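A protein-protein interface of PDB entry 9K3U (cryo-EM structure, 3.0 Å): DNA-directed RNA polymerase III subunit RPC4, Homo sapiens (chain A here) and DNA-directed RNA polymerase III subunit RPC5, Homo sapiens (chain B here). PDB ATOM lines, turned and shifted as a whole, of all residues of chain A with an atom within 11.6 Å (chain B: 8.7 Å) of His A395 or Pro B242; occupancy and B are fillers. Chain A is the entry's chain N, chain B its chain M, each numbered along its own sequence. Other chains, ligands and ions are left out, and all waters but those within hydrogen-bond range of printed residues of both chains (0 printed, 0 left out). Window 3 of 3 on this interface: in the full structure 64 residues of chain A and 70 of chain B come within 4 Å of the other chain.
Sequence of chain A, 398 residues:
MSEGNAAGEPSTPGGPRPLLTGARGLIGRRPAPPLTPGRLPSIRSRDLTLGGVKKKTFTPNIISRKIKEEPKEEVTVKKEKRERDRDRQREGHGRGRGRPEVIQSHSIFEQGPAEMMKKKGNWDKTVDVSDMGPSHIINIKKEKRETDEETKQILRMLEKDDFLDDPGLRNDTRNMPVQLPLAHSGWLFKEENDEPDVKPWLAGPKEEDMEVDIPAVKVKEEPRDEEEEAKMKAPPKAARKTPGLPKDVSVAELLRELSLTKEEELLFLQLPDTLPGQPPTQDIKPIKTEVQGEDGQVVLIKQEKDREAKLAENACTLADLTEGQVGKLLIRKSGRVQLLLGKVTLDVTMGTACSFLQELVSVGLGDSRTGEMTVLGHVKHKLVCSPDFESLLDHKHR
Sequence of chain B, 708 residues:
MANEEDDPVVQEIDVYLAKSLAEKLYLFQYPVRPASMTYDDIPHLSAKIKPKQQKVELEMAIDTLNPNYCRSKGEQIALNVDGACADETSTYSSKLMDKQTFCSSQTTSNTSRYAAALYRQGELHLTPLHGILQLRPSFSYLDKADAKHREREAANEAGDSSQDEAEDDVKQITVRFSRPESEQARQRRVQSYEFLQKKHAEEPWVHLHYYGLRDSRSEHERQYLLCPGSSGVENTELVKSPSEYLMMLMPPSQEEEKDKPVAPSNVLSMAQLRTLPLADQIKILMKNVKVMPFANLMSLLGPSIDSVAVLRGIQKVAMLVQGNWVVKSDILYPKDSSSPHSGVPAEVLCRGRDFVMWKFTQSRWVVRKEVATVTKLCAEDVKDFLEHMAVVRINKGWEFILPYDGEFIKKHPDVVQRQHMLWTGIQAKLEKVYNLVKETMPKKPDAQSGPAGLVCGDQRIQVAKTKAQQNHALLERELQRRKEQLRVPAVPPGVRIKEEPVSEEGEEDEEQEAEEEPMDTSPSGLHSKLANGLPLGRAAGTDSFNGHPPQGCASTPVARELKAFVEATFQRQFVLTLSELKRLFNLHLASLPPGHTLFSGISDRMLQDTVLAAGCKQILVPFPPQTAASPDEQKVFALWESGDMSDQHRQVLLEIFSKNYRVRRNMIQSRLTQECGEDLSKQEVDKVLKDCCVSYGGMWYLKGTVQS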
ATOM      1  N   THR A 274     -21.421 -14.994 -11.737  1.00  0.00           N
ATOM      2  CA  THR A 274     -20.427 -15.913 -11.200  1.00  0.00           C
ATOM      3  C   THR A 274     -21.035 -17.302 -11.081  1.00  0.00           C
ATOM      4  O   THR A 274     -22.098 -17.470 -10.474  1.00  0.00           O
ATOM      5  CB  THR A 274     -19.924 -15.444  -9.830  1.00  0.00           C
ATOM      6  OG1 THR A 274     -21.007 -15.449  -8.893  1.00  0.00           O
ATOM      7  CG2 THR A 274     -19.347 -14.039  -9.927  1.00  0.00           C
ATOM      8  N   LEU A 275     -20.351 -18.306 -11.667  1.00  0.00           N
ATOM      9  CA  LEU A 275     -20.818 -19.680 -11.575  1.00  0.00           C
ATOM     10  C   LEU A 275     -20.277 -20.348 -10.316  1.00  0.00           C
ATOM     11  O   LEU A 275     -19.257 -19.920  -9.765  1.00  0.00           O
ATOM     12  CB  LEU A 275     -20.380 -20.475 -12.804  1.00  0.00           C
ATOM     13  CG  LEU A 275     -21.234 -20.300 -14.064  1.00  0.00           C
ATOM     14  CD1 LEU A 275     -21.213 -18.860 -14.553  1.00  0.00           C
ATOM     15  CD2 LEU A 275     -20.765 -21.247 -15.159  1.00  0.00           C
ATOM     16  N   PRO A 276     -20.943 -21.403  -9.834  1.00  0.00           N
ATOM     17  CA  PRO A 276     -20.491 -22.062  -8.603  1.00  0.00           C
ATOM     18  C   PRO A 276     -19.260 -22.929  -8.817  1.00  0.00           C
ATOM     19  O   PRO A 276     -19.311 -24.146  -8.618  1.00  0.00           O
ATOM     20  CB  PRO A 276     -21.710 -22.899  -8.197  1.00  0.00           C
ATOM     21  CG  PRO A 276     -22.367 -23.230  -9.490  1.00  0.00           C
ATOM     22  CD  PRO A 276     -22.161 -22.030 -10.381  1.00  0.00           C
ATOM     23  N   GLY A 277     -18.150 -22.316  -9.219  1.00  0.00           N
ATOM     24  CA  GLY A 277     -16.935 -23.068  -9.463  1.00  0.00           C
ATOM     25  C   GLY A 277     -15.713 -22.186  -9.316  1.00  0.00           C
ATOM     26  O   GLY A 277     -15.808 -20.996  -9.016  1.00  0.00           O
ATOM     27  N   LEU A 339     -31.635 -26.378 -13.027  1.00  0.00           N
ATOM     28  CA  LEU A 339     -30.341 -26.663 -13.640  1.00  0.00           C
ATOM     29  C   LEU A 339     -29.382 -27.049 -12.523  1.00  0.00           C
ATOM     30  O   LEU A 339     -29.004 -26.203 -11.705  1.00  0.00           O
ATOM     31  CB  LEU A 339     -29.820 -25.453 -14.417  1.00  0.00           C
ATOM     32  CG  LEU A 339     -28.480 -25.616 -15.138  1.00  0.00           C
ATOM     33  CD1 LEU A 339     -28.621 -26.518 -16.352  1.00  0.00           C
ATOM     34  CD2 LEU A 339     -27.922 -24.259 -15.540  1.00  0.00           C
ATOM     35  N   LEU A 340     -29.006 -28.326 -12.477  1.00  0.00           N
ATOM     36  CA  LEU A 340     -28.068 -28.835 -11.481  1.00  0.00           C
ATOM     37  C   LEU A 340     -26.665 -28.693 -12.056  1.00  0.00           C
ATOM     38  O   LEU A 340     -26.235 -29.499 -12.887  1.00  0.00           O
ATOM     39  CB  LEU A 340     -28.395 -30.281 -11.125  1.00  0.00           C
ATOM     40  CG  LEU A 340     -27.591 -30.922  -9.992  1.00  0.00           C
ATOM     41  CD1 LEU A 340     -28.431 -31.965  -9.274  1.00  0.00           C
ATOM     42  CD2 LEU A 340     -26.307 -31.550 -10.512  1.00  0.00           C
ATOM     43  N   LEU A 341     -25.952 -27.658 -11.619  1.00  0.00           N
ATOM     44  CA  LEU A 341     -24.610 -27.347 -12.098  1.00  0.00           C
ATOM     45  C   LEU A 341     -23.561 -27.675 -11.040  1.00  0.00           C
ATOM     46  O   LEU A 341     -22.556 -26.977 -10.899  1.00  0.00           O
ATOM     47  CB  LEU A 341     -24.519 -25.880 -12.510  1.00  0.00           C
ATOM     48  CG  LEU A 341     -23.341 -25.476 -13.401  1.00  0.00           C
ATOM     49  CD1 LEU A 341     -23.458 -26.113 -14.776  1.00  0.00           C
ATOM     50  CD2 LEU A 341     -23.261 -23.964 -13.518  1.00  0.00           C
ATOM     51  N   GLY A 342     -23.792 -28.747 -10.285  1.00  0.00           N
ATOM     52  CA  GLY A 342     -22.887 -29.150  -9.226  1.00  0.00           C
ATOM     53  C   GLY A 342     -23.615 -29.441  -7.930  1.00  0.00           C
ATOM     54  O   GLY A 342     -24.572 -30.220  -7.910  1.00  0.00           O
ATOM     55  N   LYS A 343     -23.168 -28.819  -6.836  1.00  0.00           N
ATOM     56  CA  LYS A 343     -23.839 -28.999  -5.554  1.00  0.00           C
ATOM     57  C   LYS A 343     -25.047 -28.085  -5.407  1.00  0.00           C
ATOM     58  O   LYS A 343     -25.950 -28.382  -4.619  1.00  0.00           O
ATOM     59  CB  LYS A 343     -22.856 -28.756  -4.407  1.00  0.00           C
ATOM     60  CG  LYS A 343     -21.754 -29.797  -4.307  1.00  0.00           C
ATOM     61  CD  LYS A 343     -20.844 -29.530  -3.118  1.00  0.00           C
ATOM     62  CE  LYS A 343     -19.824 -30.643  -2.937  1.00  0.00           C
ATOM     63  NZ  LYS A 343     -18.941 -30.799  -4.125  1.00  0.00           N
ATOM     64  N   VAL A 344     -25.082 -26.981  -6.148  1.00  0.00           N
ATOM     65  CA  VAL A 344     -26.198 -26.052  -6.113  1.00  0.00           C
ATOM     66  C   VAL A 344     -27.091 -26.319  -7.315  1.00  0.00           C
ATOM     67  O   VAL A 344     -26.719 -27.018  -8.262  1.00  0.00           O
ATOM     68  CB  VAL A 344     -25.721 -24.581  -6.089  1.00  0.00           C
ATOM     69  CG1 VAL A 344     -24.771 -24.348  -4.925  1.00  0.00           C
ATOM     70  CG2 VAL A 344     -25.066 -24.209  -7.411  1.00  0.00           C
ATOM     71  N   THR A 345     -28.295 -25.751  -7.279  1.00  0.00           N
ATOM     72  CA  THR A 345     -29.278 -25.921  -8.343  1.00  0.00           C
ATOM     73  C   THR A 345     -29.925 -24.577  -8.635  1.00  0.00           C
ATOM     74  O   THR A 345     -30.592 -24.007  -7.766  1.00  0.00           O
ATOM     75  CB  THR A 345     -30.342 -26.955  -7.956  1.00  0.00           C
ATOM     76  OG1 THR A 345     -30.995 -26.543  -6.747  1.00  0.00           O
ATOM     77  CG2 THR A 345     -29.710 -28.324  -7.750  1.00  0.00           C
ATOM     78  N   LEU A 346     -29.730 -24.079  -9.849  1.00  0.00           N
ATOM     79  CA  LEU A 346     -30.369 -22.850 -10.292  1.00  0.00           C
ATOM     80  C   LEU A 346     -31.744 -23.168 -10.876  1.00  0.00           C
ATOM     81  O   LEU A 346     -32.102 -24.327 -11.087  1.00  0.00           O
ATOM     82  CB  LEU A 346     -29.500 -22.138 -11.329  1.00  0.00           C
ATOM     83  CG  LEU A 346     -27.984 -22.174 -11.106  1.00  0.00           C
ATOM     84  CD1 LEU A 346     -27.267 -21.496 -12.262  1.00  0.00           C
ATOM     85  CD2 LEU A 346     -27.596 -21.527  -9.785  1.00  0.00           C
ATOM     86  N   PRO A 387     -29.890 -18.081  -9.523  1.00  0.00           N
ATOM     87  CA  PRO A 387     -29.637 -18.904  -8.336  1.00  0.00           C
ATOM     88  C   PRO A 387     -30.872 -19.005  -7.454  1.00  0.00           C
ATOM     89  O   PRO A 387     -31.618 -18.039  -7.284  1.00  0.00           O
ATOM     90  CB  PRO A 387     -28.497 -18.167  -7.620  1.00  0.00           C
ATOM     91  CG  PRO A 387     -27.879 -17.301  -8.657  1.00  0.00           C
ATOM     92  CD  PRO A 387     -28.989 -16.919  -9.581  1.00  0.00           C
ATOM     93  N   ASP A 388     -31.081 -20.195  -6.890  1.00  0.00           N
ATOM     94  CA  ASP A 388     -32.185 -20.432  -5.961  1.00  0.00           C
ATOM     95  C   ASP A 388     -31.760 -19.921  -4.587  1.00  0.00           C
ATOM     96  O   ASP A 388     -31.351 -20.672  -3.697  1.00  0.00           O
ATOM     97  CB  ASP A 388     -32.556 -21.910  -5.930  1.00  0.00           C
ATOM     98  CG  ASP A 388     -33.778 -22.188  -5.073  1.00  0.00           C
ATOM     99  OD1 ASP A 388     -34.357 -21.225  -4.527  1.00  0.00           O
ATOM    100  OD2 ASP A 388     -34.158 -23.369  -4.948  1.00  0.00           O
ATOM    101  N   PHE A 389     -31.861 -18.599  -4.420  1.00  0.00           N
ATOM    102  CA  PHE A 389     -31.412 -17.973  -3.181  1.00  0.00           C
ATOM    103  C   PHE A 389     -32.168 -18.506  -1.974  1.00  0.00           C
ATOM    104  O   PHE A 389     -31.596 -18.611  -0.884  1.00  0.00           O
ATOM    105  CB  PHE A 389     -31.568 -16.454  -3.278  1.00  0.00           C
ATOM    106  CG  PHE A 389     -30.649 -15.814  -4.278  1.00  0.00           C
ATOM    107  CD1 PHE A 389     -29.379 -15.402  -3.905  1.00  0.00           C
ATOM    108  CD2 PHE A 389     -31.050 -15.625  -5.588  1.00  0.00           C
ATOM    109  CE1 PHE A 389     -28.530 -14.813  -4.822  1.00  0.00           C
ATOM    110  CE2 PHE A 389     -30.205 -15.038  -6.509  1.00  0.00           C
ATOM    111  CZ  PHE A 389     -28.944 -14.630  -6.125  1.00  0.00           C
ATOM    112  N   GLU A 390     -33.444 -18.856  -2.141  1.00  0.00           N
ATOM    113  CA  GLU A 390     -34.197 -19.434  -1.032  1.00  0.00           C
ATOM    114  C   GLU A 390     -33.534 -20.716  -0.539  1.00  0.00           C
ATOM    115  O   GLU A 390     -33.340 -20.907   0.668  1.00  0.00           O
ATOM    116  CB  GLU A 390     -35.639 -19.702  -1.463  1.00  0.00           C
ATOM    117  CG  GLU A 390     -36.532 -20.234  -0.352  1.00  0.00           C
ATOM    118  CD  GLU A 390     -37.965 -20.435  -0.802  1.00  0.00           C
ATOM    119  OE1 GLU A 390     -38.262 -20.164  -1.985  1.00  0.00           O
ATOM    120  OE2 GLU A 390     -38.795 -20.866   0.026  1.00  0.00           O
ATOM    121  N   SER A 391     -33.176 -21.608  -1.467  1.00  0.00           N
ATOM    122  CA  SER A 391     -32.500 -22.842  -1.087  1.00  0.00           C
ATOM    123  C   SER A 391     -31.123 -22.556  -0.505  1.00  0.00           C
ATOM    124  O   SER A 391     -30.727 -23.162   0.498  1.00  0.00           O
ATOM    125  CB  SER A 391     -32.386 -23.770  -2.296  1.00  0.00           C
ATOM    126  OG  SER A 391     -31.531 -23.216  -3.281  1.00  0.00           O
ATOM    127  N   LEU A 392     -30.372 -21.642  -1.127  1.00  0.00           N
ATOM    128  CA  LEU A 392     -29.040 -21.319  -0.625  1.00  0.00           C
ATOM    129  C   LEU A 392     -29.099 -20.768   0.793  1.00  0.00           C
ATOM    130  O   LEU A 392     -28.153 -20.948   1.570  1.00  0.00           O
ATOM    131  CB  LEU A 392     -28.357 -20.316  -1.554  1.00  0.00           C
ATOM    132  CG  LEU A 392     -28.133 -20.769  -3.000  1.00  0.00           C
ATOM    133  CD1 LEU A 392     -27.520 -19.646  -3.820  1.00  0.00           C
ATOM    134  CD2 LEU A 392     -27.260 -22.012  -3.053  1.00  0.00           C
ATOM    135  N   LEU A 393     -30.194 -20.093   1.149  1.00  0.00           N
ATOM    136  CA  LEU A 393     -30.321 -19.536   2.490  1.00  0.00           C
ATOM    137  C   LEU A 393     -30.811 -20.575   3.487  1.00  0.00           C
ATOM    138  O   LEU A 393     -30.289 -20.656   4.607  1.00  0.00           O
ATOM    139  CB  LEU A 393     -31.269 -18.334   2.471  1.00  0.00           C
ATOM    140  CG  LEU A 393     -30.762 -17.086   1.743  1.00  0.00           C
ATOM    141  CD1 LEU A 393     -31.863 -16.039   1.659  1.00  0.00           C
ATOM    142  CD2 LEU A 393     -29.532 -16.516   2.430  1.00  0.00           C
ATOM    143  N   ASP A 394     -31.804 -21.384   3.112  1.00  0.00           N
ATOM    144  CA  ASP A 394     -32.320 -22.391   4.032  1.00  0.00           C
ATOM    145  C   ASP A 394     -31.384 -23.582   4.192  1.00  0.00           C
ATOM    146  O   ASP A 394     -31.583 -24.381   5.113  1.00  0.00           O
ATOM    147  CB  ASP A 394     -33.701 -22.880   3.579  1.00  0.00           C
ATOM    148  CG  ASP A 394     -33.689 -23.470   2.182  1.00  0.00           C
ATOM    149  OD1 ASP A 394     -32.848 -24.350   1.906  1.00  0.00           O
ATOM    150  OD2 ASP A 394     -34.544 -23.064   1.366  1.00  0.00           O
ATOM    151  N   HIS A 395     -30.378 -23.726   3.326  1.00  0.00           N
ATOM    152  CA  HIS A 395     -29.404 -24.799   3.503  1.00  0.00           C
ATOM    153  C   HIS A 395     -28.537 -24.549   4.731  1.00  0.00           C
ATOM    154  O   HIS A 395     -28.309 -25.457   5.538  1.00  0.00           O
ATOM    155  CB  HIS A 395     -28.544 -24.933   2.248  1.00  0.00           C
ATOM    156  CG  HIS A 395     -27.569 -26.066   2.299  1.00  0.00           C
ATOM    157  ND1 HIS A 395     -26.218 -25.879   2.503  1.00  0.00           N
ATOM    158  CD2 HIS A 395     -27.747 -27.403   2.173  1.00  0.00           C
ATOM    159  CE1 HIS A 395     -25.608 -27.050   2.500  1.00  0.00           C
ATOM    160  NE2 HIS A 395     -26.513 -27.992   2.302  1.00  0.00           N
ATOM    161  N   LYS A 396     -28.042 -23.324   4.884  1.00  0.00           N
ATOM    162  CA  LYS A 396     -27.241 -22.955   6.045  1.00  0.00           C
ATOM    163  C   LYS A 396     -27.568 -21.533   6.492  1.00  0.00           C
ATOM    164  O   LYS A 396     -26.816 -20.598   6.218  1.00  0.00           O
ATOM    165  CB  LYS A 396     -25.747 -23.074   5.733  1.00  0.00           C
ATOM    166  CG  LYS A 396     -25.254 -24.505   5.598  1.00  0.00           C
ATOM    167  CD  LYS A 396     -23.766 -24.548   5.290  1.00  0.00           C
ATOM    168  CE  LYS A 396     -23.250 -25.976   5.226  1.00  0.00           C
ATOM    169  NZ  LYS A 396     -21.792 -26.028   4.922  1.00  0.00           N
ATOM    170  N   VAL B 239     -17.774 -27.750  -8.068  1.00  0.00           N
ATOM    171  CA  VAL B 239     -18.000 -28.640  -6.936  1.00  0.00           C
ATOM    172  C   VAL B 239     -17.993 -27.876  -5.614  1.00  0.00           C
ATOM    173  O   VAL B 239     -17.786 -28.467  -4.557  1.00  0.00           O
ATOM    174  CB  VAL B 239     -16.969 -29.784  -6.920  1.00  0.00           C
ATOM    175  CG1 VAL B 239     -17.032 -30.574  -8.223  1.00  0.00           C
ATOM    176  CG2 VAL B 239     -15.566 -29.238  -6.668  1.00  0.00           C
ATOM    177  N   LYS B 240     -18.215 -26.565  -5.654  1.00  0.00           N
ATOM    178  CA  LYS B 240     -18.267 -25.775  -4.433  1.00  0.00           C
ATOM    179  C   LYS B 240     -19.623 -25.924  -3.756  1.00  0.00           C
ATOM    180  O   LYS B 240     -20.646 -26.161  -4.406  1.00  0.00           O
ATOM    181  CB  LYS B 240     -17.991 -24.302  -4.726  1.00  0.00           C
ATOM    182  CG  LYS B 240     -16.546 -24.004  -5.094  1.00  0.00           C
ATOM    183  CD  LYS B 240     -16.229 -22.525  -4.950  1.00  0.00           C
ATOM    184  CE  LYS B 240     -14.770 -22.238  -5.257  1.00  0.00           C
ATOM    185  NZ  LYS B 240     -14.398 -20.827  -4.959  1.00  0.00           N
ATOM    186  N   SER B 241     -19.623 -25.782  -2.434  1.00  0.00           N
ATOM    187  CA  SER B 241     -20.837 -25.948  -1.661  1.00  0.00           C
ATOM    188  C   SER B 241     -21.744 -24.728  -1.815  1.00  0.00           C
ATOM    189  O   SER B 241     -21.313 -23.673  -2.291  1.00  0.00           O
ATOM    190  CB  SER B 241     -20.501 -26.168  -0.188  1.00  0.00           C
ATOM    191  OG  SER B 241     -19.815 -25.052   0.350  1.00  0.00           O
ATOM    192  N   PRO B 242     -23.016 -24.856  -1.429  1.00  0.00           N
ATOM    193  CA  PRO B 242     -23.912 -23.687  -1.494  1.00  0.00           C
ATOM    194  C   PRO B 242     -23.415 -22.505  -0.685  1.00  0.00           C
ATOM    195  O   PRO B 242     -23.566 -21.360  -1.125  1.00  0.00           O
ATOM    196  CB  PRO B 242     -25.238 -24.234  -0.945  1.00  0.00           C
ATOM    197  CG  PRO B 242     -25.171 -25.703  -1.176  1.00  0.00           C
ATOM    198  CD  PRO B 242     -23.728 -26.074  -1.010  1.00  0.00           C
ATOM    199  N   SER B 243     -22.821 -22.746   0.486  1.00  0.00           N
ATOM    200  CA  SER B 243     -22.303 -21.640   1.285  1.00  0.00           C
ATOM    201  C   SER B 243     -21.166 -20.927   0.565  1.00  0.00           C
ATOM    202  O   SER B 243     -21.107 -19.691   0.553  1.00  0.00           O
ATOM    203  CB  SER B 243     -21.834 -22.156   2.647  1.00  0.00           C
ATOM    204  OG  SER B 243     -21.317 -21.101   3.440  1.00  0.00           O
ATOM    205  N   GLU B 244     -20.253 -21.689  -0.041  1.00  0.00           N
ATOM    206  CA  GLU B 244     -19.166 -21.072  -0.795  1.00  0.00           C
ATOM    207  C   GLU B 244     -19.703 -20.291  -1.987  1.00  0.00           C
ATOM    208  O   GLU B 244     -19.233 -19.184  -2.276  1.00  0.00           O
ATOM    209  CB  GLU B 244     -18.176 -22.141  -1.255  1.00  0.00           C
ATOM    210  CG  GLU B 244     -17.458 -22.849  -0.116  1.00  0.00           C
ATOM    211  CD  GLU B 244     -16.503 -23.919  -0.605  1.00  0.00           C
ATOM    212  OE1 GLU B 244     -16.397 -24.107  -1.836  1.00  0.00           O
ATOM    213  OE2 GLU B 244     -15.853 -24.569   0.242  1.00  0.00           O
ATOM    214  N   TYR B 245     -20.692 -20.848  -2.690  1.00  0.00           N
ATOM    215  CA  TYR B 245     -21.275 -20.136  -3.823  1.00  0.00           C
ATOM    216  C   TYR B 245     -21.930 -18.837  -3.374  1.00  0.00           C
ATOM    217  O   TYR B 245     -21.821 -17.807  -4.054  1.00  0.00           O
ATOM    218  CB  TYR B 245     -22.293 -21.028  -4.535  1.00  0.00           C
ATOM    219  CG  TYR B 245     -22.878 -20.423  -5.798  1.00  0.00           C
ATOM    220  CD1 TYR B 245     -22.172 -19.484  -6.541  1.00  0.00           C
ATOM    221  CD2 TYR B 245     -24.141 -20.790  -6.242  1.00  0.00           C
ATOM    222  CE1 TYR B 245     -22.704 -18.935  -7.691  1.00  0.00           C
ATOM    223  CE2 TYR B 245     -24.682 -20.244  -7.391  1.00  0.00           C
ATOM    224  CZ  TYR B 245     -23.959 -19.317  -8.112  1.00  0.00           C
ATOM    225  OH  TYR B 245     -24.495 -18.771  -9.255  1.00  0.00           O
ATOM    226  N   LEU B 246     -22.621 -18.865  -2.231  1.00  0.00           N
ATOM    227  CA  LEU B 246     -23.254 -17.656  -1.714  1.00  0.00           C
ATOM    228  C   LEU B 246     -22.210 -16.613  -1.334  1.00  0.00           C
ATOM    229  O   LEU B 246     -22.357 -15.431  -1.665  1.00  0.00           O
ATOM    230  CB  LEU B 246     -24.133 -18.004  -0.514  1.00  0.00           C
ATOM    231  CG  LEU B 246     -24.907 -16.849   0.126  1.00  0.00           C
ATOM    232  CD1 LEU B 246     -25.833 -16.188  -0.883  1.00  0.00           C
ATOM    233  CD2 LEU B 246     -25.692 -17.343   1.331  1.00  0.00           C
ATOM    234  N   MET B 247     -21.155 -17.031  -0.629  1.00  0.00           N
ATOM    235  CA  MET B 247     -20.087 -16.099  -0.283  1.00  0.00           C
ATOM    236  C   MET B 247     -19.434 -15.517  -1.528  1.00  0.00           C
ATOM    237  O   MET B 247     -19.010 -14.354  -1.520  1.00  0.00           O
ATOM    238  CB  MET B 247     -19.037 -16.794   0.584  1.00  0.00           C
ATOM    239  CG  MET B 247     -19.538 -17.268   1.942  1.00  0.00           C
ATOM    240  SD  MET B 247     -20.104 -15.936   3.018  1.00  0.00           S
ATOM    241  CE  MET B 247     -21.859 -15.923   2.659  1.00  0.00           C
ATOM    242  N   MET B 248     -19.339 -16.302  -2.603  1.00  0.00           N
ATOM    243  CA  MET B 248     -18.752 -15.799  -3.838  1.00  0.00           C
ATOM    244  C   MET B 248     -19.660 -14.763  -4.493  1.00  0.00           C
ATOM    245  O   MET B 248     -19.213 -13.662  -4.837  1.00  0.00           O
ATOM    246  CB  MET B 248     -18.480 -16.958  -4.798  1.00  0.00           C
ATOM    247  CG  MET B 248     -17.811 -16.545  -6.101  1.00  0.00           C
ATOM    248  SD  MET B 248     -17.623 -17.913  -7.264  1.00  0.00           S
ATOM    249  CE  MET B 248     -16.550 -19.006  -6.334  1.00  0.00           C
ATOM    250  N   LEU B 249     -20.936 -15.099  -4.675  1.00  0.00           N
ATOM    251  CA  LEU B 249     -21.856 -14.205  -5.366  1.00  0.00           C
ATOM    252  C   LEU B 249     -22.284 -13.015  -4.515  1.00  0.00           C
ATOM    253  O   LEU B 249     -22.921 -12.097  -5.046  1.00  0.00           O
ATOM    254  CB  LEU B 249     -23.094 -14.980  -5.838  1.00  0.00           C
ATOM    255  CG  LEU B 249     -23.959 -15.673  -4.782  1.00  0.00           C
ATOM    256  CD1 LEU B 249     -24.876 -14.694  -4.065  1.00  0.00           C
ATOM    257  CD2 LEU B 249     -24.768 -16.798  -5.419  1.00  0.00           C
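N of Glu B244 lies close to OG of Ser B241, 3.4 Å away.
N of Leu A339 lies within hydrogen-bond range of O of Leu A346.
The side-chain amino group of Lys A343 lies within hydrogen-bond range of the backbone carbonyl oxygen of Val B239 (2.6 Å).
The side-chain hydroxyl (OH) of Tyr B245 sits at hydrogen-bond distance from the backbone carbonyl oxygen (O) of Thr A274 (3.0 Å).
The backbone carbonyl oxygen of Leu A275 sits close to the side-chain sulfur of Met B248 (3.6 Å).
Hydrophobic or aromatic side chains of chain B within 4 Å of the printed part of chain A: Val B239, Pro B242, Tyr B245, Met B248 and Leu B249.
Hydrophobic or aromatic side chains of chain A that line the printed part of chain B: Pro A276, Val A344, Leu A346, Pro A387, Phe A389, Leu A392 and His A395.
Among the printed residues, no Asp or Glu carboxylate lies within 4 Å of a Lys or Arg side-chain nitrogen of the other chain.
Among the printed residues, merely in contact across the chains: Lys A343 with Lys B240, Gly A277 with Met B248, Val A344 with Pro B242, Pro A276 with Tyr B245, Leu A392 with Pro B242, Thr A274 with Leu B249, Val A344 with Tyr B245, Phe A389 with Leu B249, Pro A387 with Tyr B245, His A395 with Pro B242, Leu A275 with Tyr B245, Lys A343 with Ser B241, Pro A276 with Val B239, Pro A276 with Lys B240 and Leu A346 with Tyr B245.
His A395 touches just one residue of chain B: Pro B242.
Pro B242 touches three residues of chain A.
No residue of chain B comes within 4 Å of Lys A396.
No residue of chain A comes within 4 Å of Ser B243.
No residue of chain A comes within 4 Å of Leu B246.
Of the printed residues of chain A, Leu B249 touches Thr A274 (3.7 Å) and Phe A389 (3.7 Å).
Of the printed residues of chain B, Leu A275 touches Tyr B245 (3.8 Å) and Met B248 (3.6 Å).
Of the printed residues of chain B, Leu A346 touches Tyr B245.
Printed residues of chain B within 4 Å of Gly A277: Met B248.
Of the printed residues of chain B, Leu A392 touches Pro B242.
Asp A388 touches none of the printed residues of chain B.
Met B247 touches none of the printed residues of chain A.
The nearest residue of chain B that does not touch His A395 is Ser B243 (5.0 Å).
The nearest residue of chain A that does not touch Pro B242 is Lys A343 (4.4 Å).
The nearest printed residue of chain B that does not touch Thr A274 is Met B248 (4.2 Å).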
